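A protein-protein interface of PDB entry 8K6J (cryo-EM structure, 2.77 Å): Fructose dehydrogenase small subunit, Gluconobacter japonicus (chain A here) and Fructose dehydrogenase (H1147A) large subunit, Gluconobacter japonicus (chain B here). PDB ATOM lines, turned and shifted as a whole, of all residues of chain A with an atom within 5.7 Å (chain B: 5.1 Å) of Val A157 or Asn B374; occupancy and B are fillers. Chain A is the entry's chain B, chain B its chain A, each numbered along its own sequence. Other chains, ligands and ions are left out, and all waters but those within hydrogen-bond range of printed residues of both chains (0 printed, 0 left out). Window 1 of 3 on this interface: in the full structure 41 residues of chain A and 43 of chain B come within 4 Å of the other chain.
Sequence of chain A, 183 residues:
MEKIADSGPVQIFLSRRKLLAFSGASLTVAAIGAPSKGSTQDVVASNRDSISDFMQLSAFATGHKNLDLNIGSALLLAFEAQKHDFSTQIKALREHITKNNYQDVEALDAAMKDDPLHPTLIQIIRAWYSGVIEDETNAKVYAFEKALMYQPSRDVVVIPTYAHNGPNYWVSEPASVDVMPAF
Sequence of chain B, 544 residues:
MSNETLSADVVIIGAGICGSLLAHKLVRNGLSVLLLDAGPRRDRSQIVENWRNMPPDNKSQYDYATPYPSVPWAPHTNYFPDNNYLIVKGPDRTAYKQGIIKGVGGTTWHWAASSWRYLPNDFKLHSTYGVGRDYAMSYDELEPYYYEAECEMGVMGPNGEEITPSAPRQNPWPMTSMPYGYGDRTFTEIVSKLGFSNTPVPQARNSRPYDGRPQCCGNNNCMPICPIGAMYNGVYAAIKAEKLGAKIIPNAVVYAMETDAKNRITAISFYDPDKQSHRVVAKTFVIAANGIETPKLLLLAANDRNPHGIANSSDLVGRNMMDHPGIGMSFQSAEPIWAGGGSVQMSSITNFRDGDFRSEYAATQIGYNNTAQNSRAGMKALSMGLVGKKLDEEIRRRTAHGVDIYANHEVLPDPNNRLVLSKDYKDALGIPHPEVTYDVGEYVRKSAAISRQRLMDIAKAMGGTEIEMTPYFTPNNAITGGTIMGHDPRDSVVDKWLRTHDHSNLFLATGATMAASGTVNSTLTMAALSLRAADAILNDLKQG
N of Asn B374 sits at hydrogen-bond distance from OG1 of Thr B399.
Of chain B, only Trp B338, Ala B339, Ala B372, Asn B374 and Thr B399 come within 4 Å of Val A157. Printed residues of chain B within 4 Å of Ile A159: Asn B374 (3.9 Å). Of the printed residues of chain B, Pro A160 touches Asn B374. Printed residues of chain A within 4 Å of Ser B375: Tyr A150. Arg A154 touches none of the printed residues of chain B. Arg B376 touches none of the printed residues of chain A. The nearest residue of chain B that does not touch Val A157 is Gln B373 (4.6 Å). The nearest printed residue of chain A that does not touch Trp B338 is Ser A153 (4.4 Å).
Among the printed residues, pairs that only touch across the chains: Met A149 with Gly B378, Tyr A150 with Asn B374, Ser A153 with Asn B374, Ser A153 with Thr B399, Val A156 with Trp B338, Val A157 with Trp B338, Val A157 with Ala B339, Val A157 with Ala B372, Val A157 with Asn B374, Val A157 with Thr B399, Val A158 with Gly B340, Val A158 with Ala B372, Ile A159 with Asn B374 and Pro A160 with Asn B374.
OH of Tyr A150 lies close to OG of Ser B375 (2.3 Å). The side-chain amide nitrogen of Asn B374 is in hydrogen-bond range of the backbone carbonyl oxygen of Val A158, at 3.2 Å.
Hydrophobic or aromatic side chains of chain B that line the printed part of chain A: Trp B338 and Ala B372.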
ATOM      1  N   MET A 149     -13.401   2.184  25.047  1.00  0.00           N
ATOM      2  CA  MET A 149     -14.133   0.978  25.407  1.00  0.00           C
ATOM      3  C   MET A 149     -13.233  -0.123  25.947  1.00  0.00           C
ATOM      4  O   MET A 149     -13.743  -1.094  26.513  1.00  0.00           O
ATOM      5  CB  MET A 149     -14.918   0.453  24.205  1.00  0.00           C
ATOM      6  CG  MET A 149     -14.114  -0.421  23.270  1.00  0.00           C
ATOM      7  SD  MET A 149     -15.154  -1.246  22.060  1.00  0.00           S
ATOM      8  CE  MET A 149     -13.912  -1.984  21.013  1.00  0.00           C
ATOM      9  N   TYR A 150     -11.919   0.001  25.786  1.00  0.00           N
ATOM     10  CA  TYR A 150     -10.986  -0.960  26.353  1.00  0.00           C
ATOM     11  C   TYR A 150     -10.490  -0.559  27.731  1.00  0.00           C
ATOM     12  O   TYR A 150     -10.081  -1.430  28.506  1.00  0.00           O
ATOM     13  CB  TYR A 150      -9.783  -1.135  25.428  1.00  0.00           C
ATOM     14  CG  TYR A 150     -10.090  -1.828  24.128  1.00  0.00           C
ATOM     15  CD1 TYR A 150     -10.457  -3.161  24.102  1.00  0.00           C
ATOM     16  CD2 TYR A 150     -10.002  -1.151  22.923  1.00  0.00           C
ATOM     17  CE1 TYR A 150     -10.733  -3.799  22.917  1.00  0.00           C
ATOM     18  CE2 TYR A 150     -10.276  -1.781  21.732  1.00  0.00           C
ATOM     19  CZ  TYR A 150     -10.641  -3.105  21.734  1.00  0.00           C
ATOM     20  OH  TYR A 150     -10.917  -3.739  20.548  1.00  0.00           O
ATOM     21  N   SER A 153     -11.577  -2.188  31.369  1.00  0.00           N
ATOM     22  CA  SER A 153     -11.005  -3.483  31.715  1.00  0.00           C
ATOM     23  C   SER A 153      -9.508  -3.536  31.439  1.00  0.00           C
ATOM     24  O   SER A 153      -8.932  -4.624  31.379  1.00  0.00           O
ATOM     25  CB  SER A 153     -11.713  -4.605  30.962  1.00  0.00           C
ATOM     26  OG  SER A 153     -11.874  -4.275  29.596  1.00  0.00           O
ATOM     27  N   ARG A 154      -8.871  -2.378  31.263  1.00  0.00           N
ATOM     28  CA  ARG A 154      -7.445  -2.353  30.961  1.00  0.00           C
ATOM     29  C   ARG A 154      -6.618  -2.944  32.093  1.00  0.00           C
ATOM     30  O   ARG A 154      -5.553  -3.520  31.847  1.00  0.00           O
ATOM     31  CB  ARG A 154      -6.998  -0.921  30.676  1.00  0.00           C
ATOM     32  CG  ARG A 154      -5.904  -0.799  29.639  1.00  0.00           C
ATOM     33  CD  ARG A 154      -5.181   0.531  29.788  1.00  0.00           C
ATOM     34  NE  ARG A 154      -4.800   1.135  28.516  1.00  0.00           N
ATOM     35  CZ  ARG A 154      -4.000   0.579  27.615  1.00  0.00           C
ATOM     36  NH1 ARG A 154      -3.429  -0.596  27.823  1.00  0.00           N
ATOM     37  NH2 ARG A 154      -3.751   1.228  26.482  1.00  0.00           N
ATOM     38  N   ASP A 155      -7.087  -2.814  33.333  1.00  0.00           N
ATOM     39  CA  ASP A 155      -6.323  -3.293  34.475  1.00  0.00           C
ATOM     40  C   ASP A 155      -6.353  -4.807  34.618  1.00  0.00           C
ATOM     41  O   ASP A 155      -5.494  -5.365  35.307  1.00  0.00           O
ATOM     42  CB  ASP A 155      -6.841  -2.649  35.761  1.00  0.00           C
ATOM     43  CG  ASP A 155      -8.260  -3.057  36.081  1.00  0.00           C
ATOM     44  OD1 ASP A 155      -9.034  -3.302  35.136  1.00  0.00           O
ATOM     45  OD2 ASP A 155      -8.602  -3.134  37.279  1.00  0.00           O
ATOM     46  N   VAL A 156      -7.314  -5.484  33.992  1.00  0.00           N
ATOM     47  CA  VAL A 156      -7.428  -6.932  34.126  1.00  0.00           C
ATOM     48  C   VAL A 156      -7.330  -7.597  32.761  1.00  0.00           C
ATOM     49  O   VAL A 156      -6.430  -8.407  32.517  1.00  0.00           O
ATOM     50  CB  VAL A 156      -8.740  -7.324  34.825  1.00  0.00           C
ATOM     51  CG1 VAL A 156      -8.775  -8.817  35.057  1.00  0.00           C
ATOM     52  CG2 VAL A 156      -8.886  -6.578  36.136  1.00  0.00           C
ATOM     53  N   VAL A 157      -8.254  -7.269  31.869  1.00  0.00           N
ATOM     54  CA  VAL A 157      -8.299  -7.892  30.553  1.00  0.00           C
ATOM     55  C   VAL A 157      -7.251  -7.253  29.655  1.00  0.00           C
ATOM     56  O   VAL A 157      -7.102  -6.028  29.617  1.00  0.00           O
ATOM     57  CB  VAL A 157      -9.705  -7.774  29.946  1.00  0.00           C
ATOM     58  CG1 VAL A 157      -9.757  -8.463  28.599  1.00  0.00           C
ATOM     59  CG2 VAL A 157     -10.732  -8.371  30.882  1.00  0.00           C
ATOM     60  N   VAL A 158      -6.520  -8.088  28.930  1.00  0.00           N
ATOM     61  CA  VAL A 158      -5.446  -7.618  28.065  1.00  0.00           C
ATOM     62  C   VAL A 158      -6.038  -7.089  26.768  1.00  0.00           C
ATOM     63  O   VAL A 158      -6.833  -7.770  26.111  1.00  0.00           O
ATOM     64  CB  VAL A 158      -4.442  -8.746  27.791  1.00  0.00           C
ATOM     65  CG1 VAL A 158      -5.172 -10.058  27.610  1.00  0.00           C
ATOM     66  CG2 VAL A 158      -3.618  -8.433  26.558  1.00  0.00           C
ATOM     67  N   ILE A 159      -5.662  -5.869  26.400  1.00  0.00           N
ATOM     68  CA  ILE A 159      -5.920  -5.373  25.052  1.00  0.00           C
ATOM     69  C   ILE A 159      -5.128  -6.283  24.125  1.00  0.00           C
ATOM     70  O   ILE A 159      -3.893  -6.218  24.115  1.00  0.00           O
ATOM     71  CB  ILE A 159      -5.511  -3.904  24.900  1.00  0.00           C
ATOM     72  CG1 ILE A 159      -6.335  -3.033  25.846  1.00  0.00           C
ATOM     73  CG2 ILE A 159      -5.695  -3.456  23.466  1.00  0.00           C
ATOM     74  CD1 ILE A 159      -6.292  -1.575  25.513  1.00  0.00           C
ATOM     75  N   PRO A 160      -5.793  -7.119  23.320  1.00  0.00           N
ATOM     76  CA  PRO A 160      -5.165  -8.350  22.819  1.00  0.00           C
ATOM     77  C   PRO A 160      -3.741  -8.230  22.294  1.00  0.00           C
ATOM     78  O   PRO A 160      -2.828  -8.825  22.871  1.00  0.00           O
ATOM     79  CB  PRO A 160      -6.121  -8.776  21.703  1.00  0.00           C
ATOM     80  CG  PRO A 160      -7.447  -8.314  22.183  1.00  0.00           C
ATOM     81  CD  PRO A 160      -7.203  -7.017  22.910  1.00  0.00           C
ATOM     82  N   HIS A 164       0.247  -7.455  28.440  1.00  0.00           N
ATOM     83  CA  HIS A 164       0.179  -7.044  29.834  1.00  0.00           C
ATOM     84  C   HIS A 164       1.561  -7.240  30.461  1.00  0.00           C
ATOM     85  O   HIS A 164       2.542  -7.533  29.774  1.00  0.00           O
ATOM     86  CB  HIS A 164      -0.908  -7.826  30.561  1.00  0.00           C
ATOM     87  CG  HIS A 164      -1.910  -6.968  31.265  1.00  0.00           C
ATOM     88  ND1 HIS A 164      -2.241  -7.146  32.590  1.00  0.00           N
ATOM     89  CD2 HIS A 164      -2.662  -5.932  30.826  1.00  0.00           C
ATOM     90  CE1 HIS A 164      -3.149  -6.253  32.940  1.00  0.00           C
ATOM     91  NE2 HIS A 164      -3.422  -5.505  31.888  1.00  0.00           N
ATOM     92  N   TRP B 338     -13.524 -13.181  33.689  1.00  0.00           N
ATOM     93  CA  TRP B 338     -12.354 -12.411  33.268  1.00  0.00           C
ATOM     94  C   TRP B 338     -11.573 -13.137  32.173  1.00  0.00           C
ATOM     95  O   TRP B 338     -10.372 -13.384  32.283  1.00  0.00           O
ATOM     96  CB  TRP B 338     -11.455 -12.098  34.465  1.00  0.00           C
ATOM     97  CG  TRP B 338     -12.040 -11.108  35.414  1.00  0.00           C
ATOM     98  CD1 TRP B 338     -12.408 -11.332  36.705  1.00  0.00           C
ATOM     99  CD2 TRP B 338     -12.319  -9.731  35.150  1.00  0.00           C
ATOM    100  NE1 TRP B 338     -12.901 -10.180  37.263  1.00  0.00           N
ATOM    101  CE2 TRP B 338     -12.857  -9.182  36.327  1.00  0.00           C
ATOM    102  CE3 TRP B 338     -12.168  -8.909  34.032  1.00  0.00           C
ATOM    103  CZ2 TRP B 338     -13.243  -7.851  36.418  1.00  0.00           C
ATOM    104  CZ3 TRP B 338     -12.552  -7.590  34.124  1.00  0.00           C
ATOM    105  CH2 TRP B 338     -13.083  -7.072  35.308  1.00  0.00           C
ATOM    106  N   ALA B 339     -12.287 -13.483  31.106  1.00  0.00           N
ATOM    107  CA  ALA B 339     -11.668 -14.196  29.998  1.00  0.00           C
ATOM    108  C   ALA B 339     -10.609 -13.333  29.328  1.00  0.00           C
ATOM    109  O   ALA B 339     -10.814 -12.138  29.097  1.00  0.00           O
ATOM    110  CB  ALA B 339     -12.726 -14.609  28.979  1.00  0.00           C
ATOM    111  N   GLY B 340      -9.470 -13.942  29.015  1.00  0.00           N
ATOM    112  CA  GLY B 340      -8.423 -13.231  28.312  1.00  0.00           C
ATOM    113  C   GLY B 340      -7.028 -13.464  28.850  1.00  0.00           C
ATOM    114  O   GLY B 340      -6.044 -13.083  28.212  1.00  0.00           O
ATOM    115  N   ALA B 372     -10.175 -12.670  24.721  1.00  0.00           N
ATOM    116  CA  ALA B 372     -10.599 -11.518  25.500  1.00  0.00           C
ATOM    117  C   ALA B 372     -11.933 -10.989  24.990  1.00  0.00           C
ATOM    118  O   ALA B 372     -12.164 -10.899  23.783  1.00  0.00           O
ATOM    119  CB  ALA B 372      -9.540 -10.420  25.440  1.00  0.00           C
ATOM    120  N   GLN B 373     -12.815 -10.642  25.922  1.00  0.00           N
ATOM    121  CA  GLN B 373     -14.160 -10.198  25.591  1.00  0.00           C
ATOM    122  C   GLN B 373     -14.316  -8.687  25.641  1.00  0.00           C
ATOM    123  O   GLN B 373     -15.444  -8.193  25.584  1.00  0.00           O
ATOM    124  CB  GLN B 373     -15.173 -10.851  26.530  1.00  0.00           C
ATOM    125  CG  GLN B 373     -15.261 -12.354  26.385  1.00  0.00           C
ATOM    126  CD  GLN B 373     -16.521 -12.793  25.680  1.00  0.00           C
ATOM    127  OE1 GLN B 373     -17.602 -12.261  25.928  1.00  0.00           O
ATOM    128  NE2 GLN B 373     -16.390 -13.764  24.787  1.00  0.00           N
ATOM    129  N   ASN B 374     -13.214  -7.941  25.751  1.00  0.00           N
ATOM    130  CA  ASN B 374     -13.322  -6.489  25.867  1.00  0.00           C
ATOM    131  C   ASN B 374     -13.913  -5.873  24.606  1.00  0.00           C
ATOM    132  O   ASN B 374     -14.738  -4.957  24.686  1.00  0.00           O
ATOM    133  CB  ASN B 374     -11.956  -5.880  26.177  1.00  0.00           C
ATOM    134  CG  ASN B 374     -10.849  -6.493  25.359  1.00  0.00           C
ATOM    135  OD1 ASN B 374     -11.098  -7.145  24.348  1.00  0.00           O
ATOM    136  ND2 ASN B 374      -9.613  -6.288  25.791  1.00  0.00           N
ATOM    137  N   SER B 375     -13.505  -6.357  23.432  1.00  0.00           N
ATOM    138  CA  SER B 375     -14.068  -5.841  22.188  1.00  0.00           C
ATOM    139  C   SER B 375     -15.553  -6.162  22.087  1.00  0.00           C
ATOM    140  O   SER B 375     -16.373  -5.291  21.766  1.00  0.00           O
ATOM    141  CB  SER B 375     -13.312  -6.419  20.993  1.00  0.00           C
ATOM    142  OG  SER B 375     -12.101  -5.721  20.770  1.00  0.00           O
ATOM    143  N   ARG B 376     -15.918  -7.415  22.365  1.00  0.00           N
ATOM    144  CA  ARG B 376     -17.320  -7.807  22.313  1.00  0.00           C
ATOM    145  C   ARG B 376     -18.142  -7.038  23.335  1.00  0.00           C
ATOM    146  O   ARG B 376     -19.242  -6.563  23.028  1.00  0.00           O
ATOM    147  CB  ARG B 376     -17.448  -9.309  22.548  1.00  0.00           C
ATOM    148  CG  ARG B 376     -18.856  -9.770  22.855  1.00  0.00           C
ATOM    149  CD  ARG B 376     -19.449 -10.495  21.669  1.00  0.00           C
ATOM    150  NE  ARG B 376     -18.464 -11.349  21.021  1.00  0.00           N
ATOM    151  CZ  ARG B 376     -18.321 -12.642  21.266  1.00  0.00           C
ATOM    152  NH1 ARG B 376     -19.091 -13.268  22.139  1.00  0.00           N
ATOM    153  NH2 ARG B 376     -17.383 -13.326  20.620  1.00  0.00           N
ATOM    154  N   ALA B 377     -17.621  -6.900  24.555  1.00  0.00           N
ATOM    155  CA  ALA B 377     -18.341  -6.169  25.589  1.00  0.00           C
ATOM    156  C   ALA B 377     -18.529  -4.712  25.205  1.00  0.00           C
ATOM    157  O   ALA B 377     -19.612  -4.149  25.391  1.00  0.00           O
ATOM    158  CB  ALA B 377     -17.597  -6.272  26.914  1.00  0.00           C
ATOM    159  N   GLY B 378     -17.484  -4.081  24.670  1.00  0.00           N
ATOM    160  CA  GLY B 378     -17.604  -2.689  24.274  1.00  0.00           C
ATOM    161  C   GLY B 378     -18.619  -2.493  23.167  1.00  0.00           C
ATOM    162  O   GLY B 378     -19.454  -1.587  23.227  1.00  0.00           O
ATOM    163  N   MET B 379     -18.568  -3.349  22.145  1.00  0.00           N
ATOM    164  CA  MET B 379     -19.522  -3.228  21.049  1.00  0.00           C
ATOM    165  C   MET B 379     -20.949  -3.459  21.530  1.00  0.00           C
ATOM    166  O   MET B 379     -21.865  -2.717  21.154  1.00  0.00           O
ATOM    167  CB  MET B 379     -19.163  -4.204  19.931  1.00  0.00           C
ATOM    168  CG  MET B 379     -17.963  -3.774  19.112  1.00  0.00           C
ATOM    169  SD  MET B 379     -17.778  -1.984  19.064  1.00  0.00           S
ATOM    170  CE  MET B 379     -18.460  -1.618  17.453  1.00  0.00           C
ATOM    171  N   THR B 399     -17.372  -7.451  29.944  1.00  0.00           N
ATOM    172  CA  THR B 399     -16.069  -8.042  29.678  1.00  0.00           C
ATOM    173  C   THR B 399     -15.587  -8.922  30.820  1.00  0.00           C
ATOM    174  O   THR B 399     -14.664  -9.718  30.623  1.00  0.00           O
ATOM    175  CB  THR B 399     -15.032  -6.958  29.401  1.00  0.00           C
ATOM    176  OG1 THR B 399     -13.822  -7.565  28.936  1.00  0.00           O
ATOM    177  CG2 THR B 399     -14.735  -6.194  30.655  1.00  0.00           C
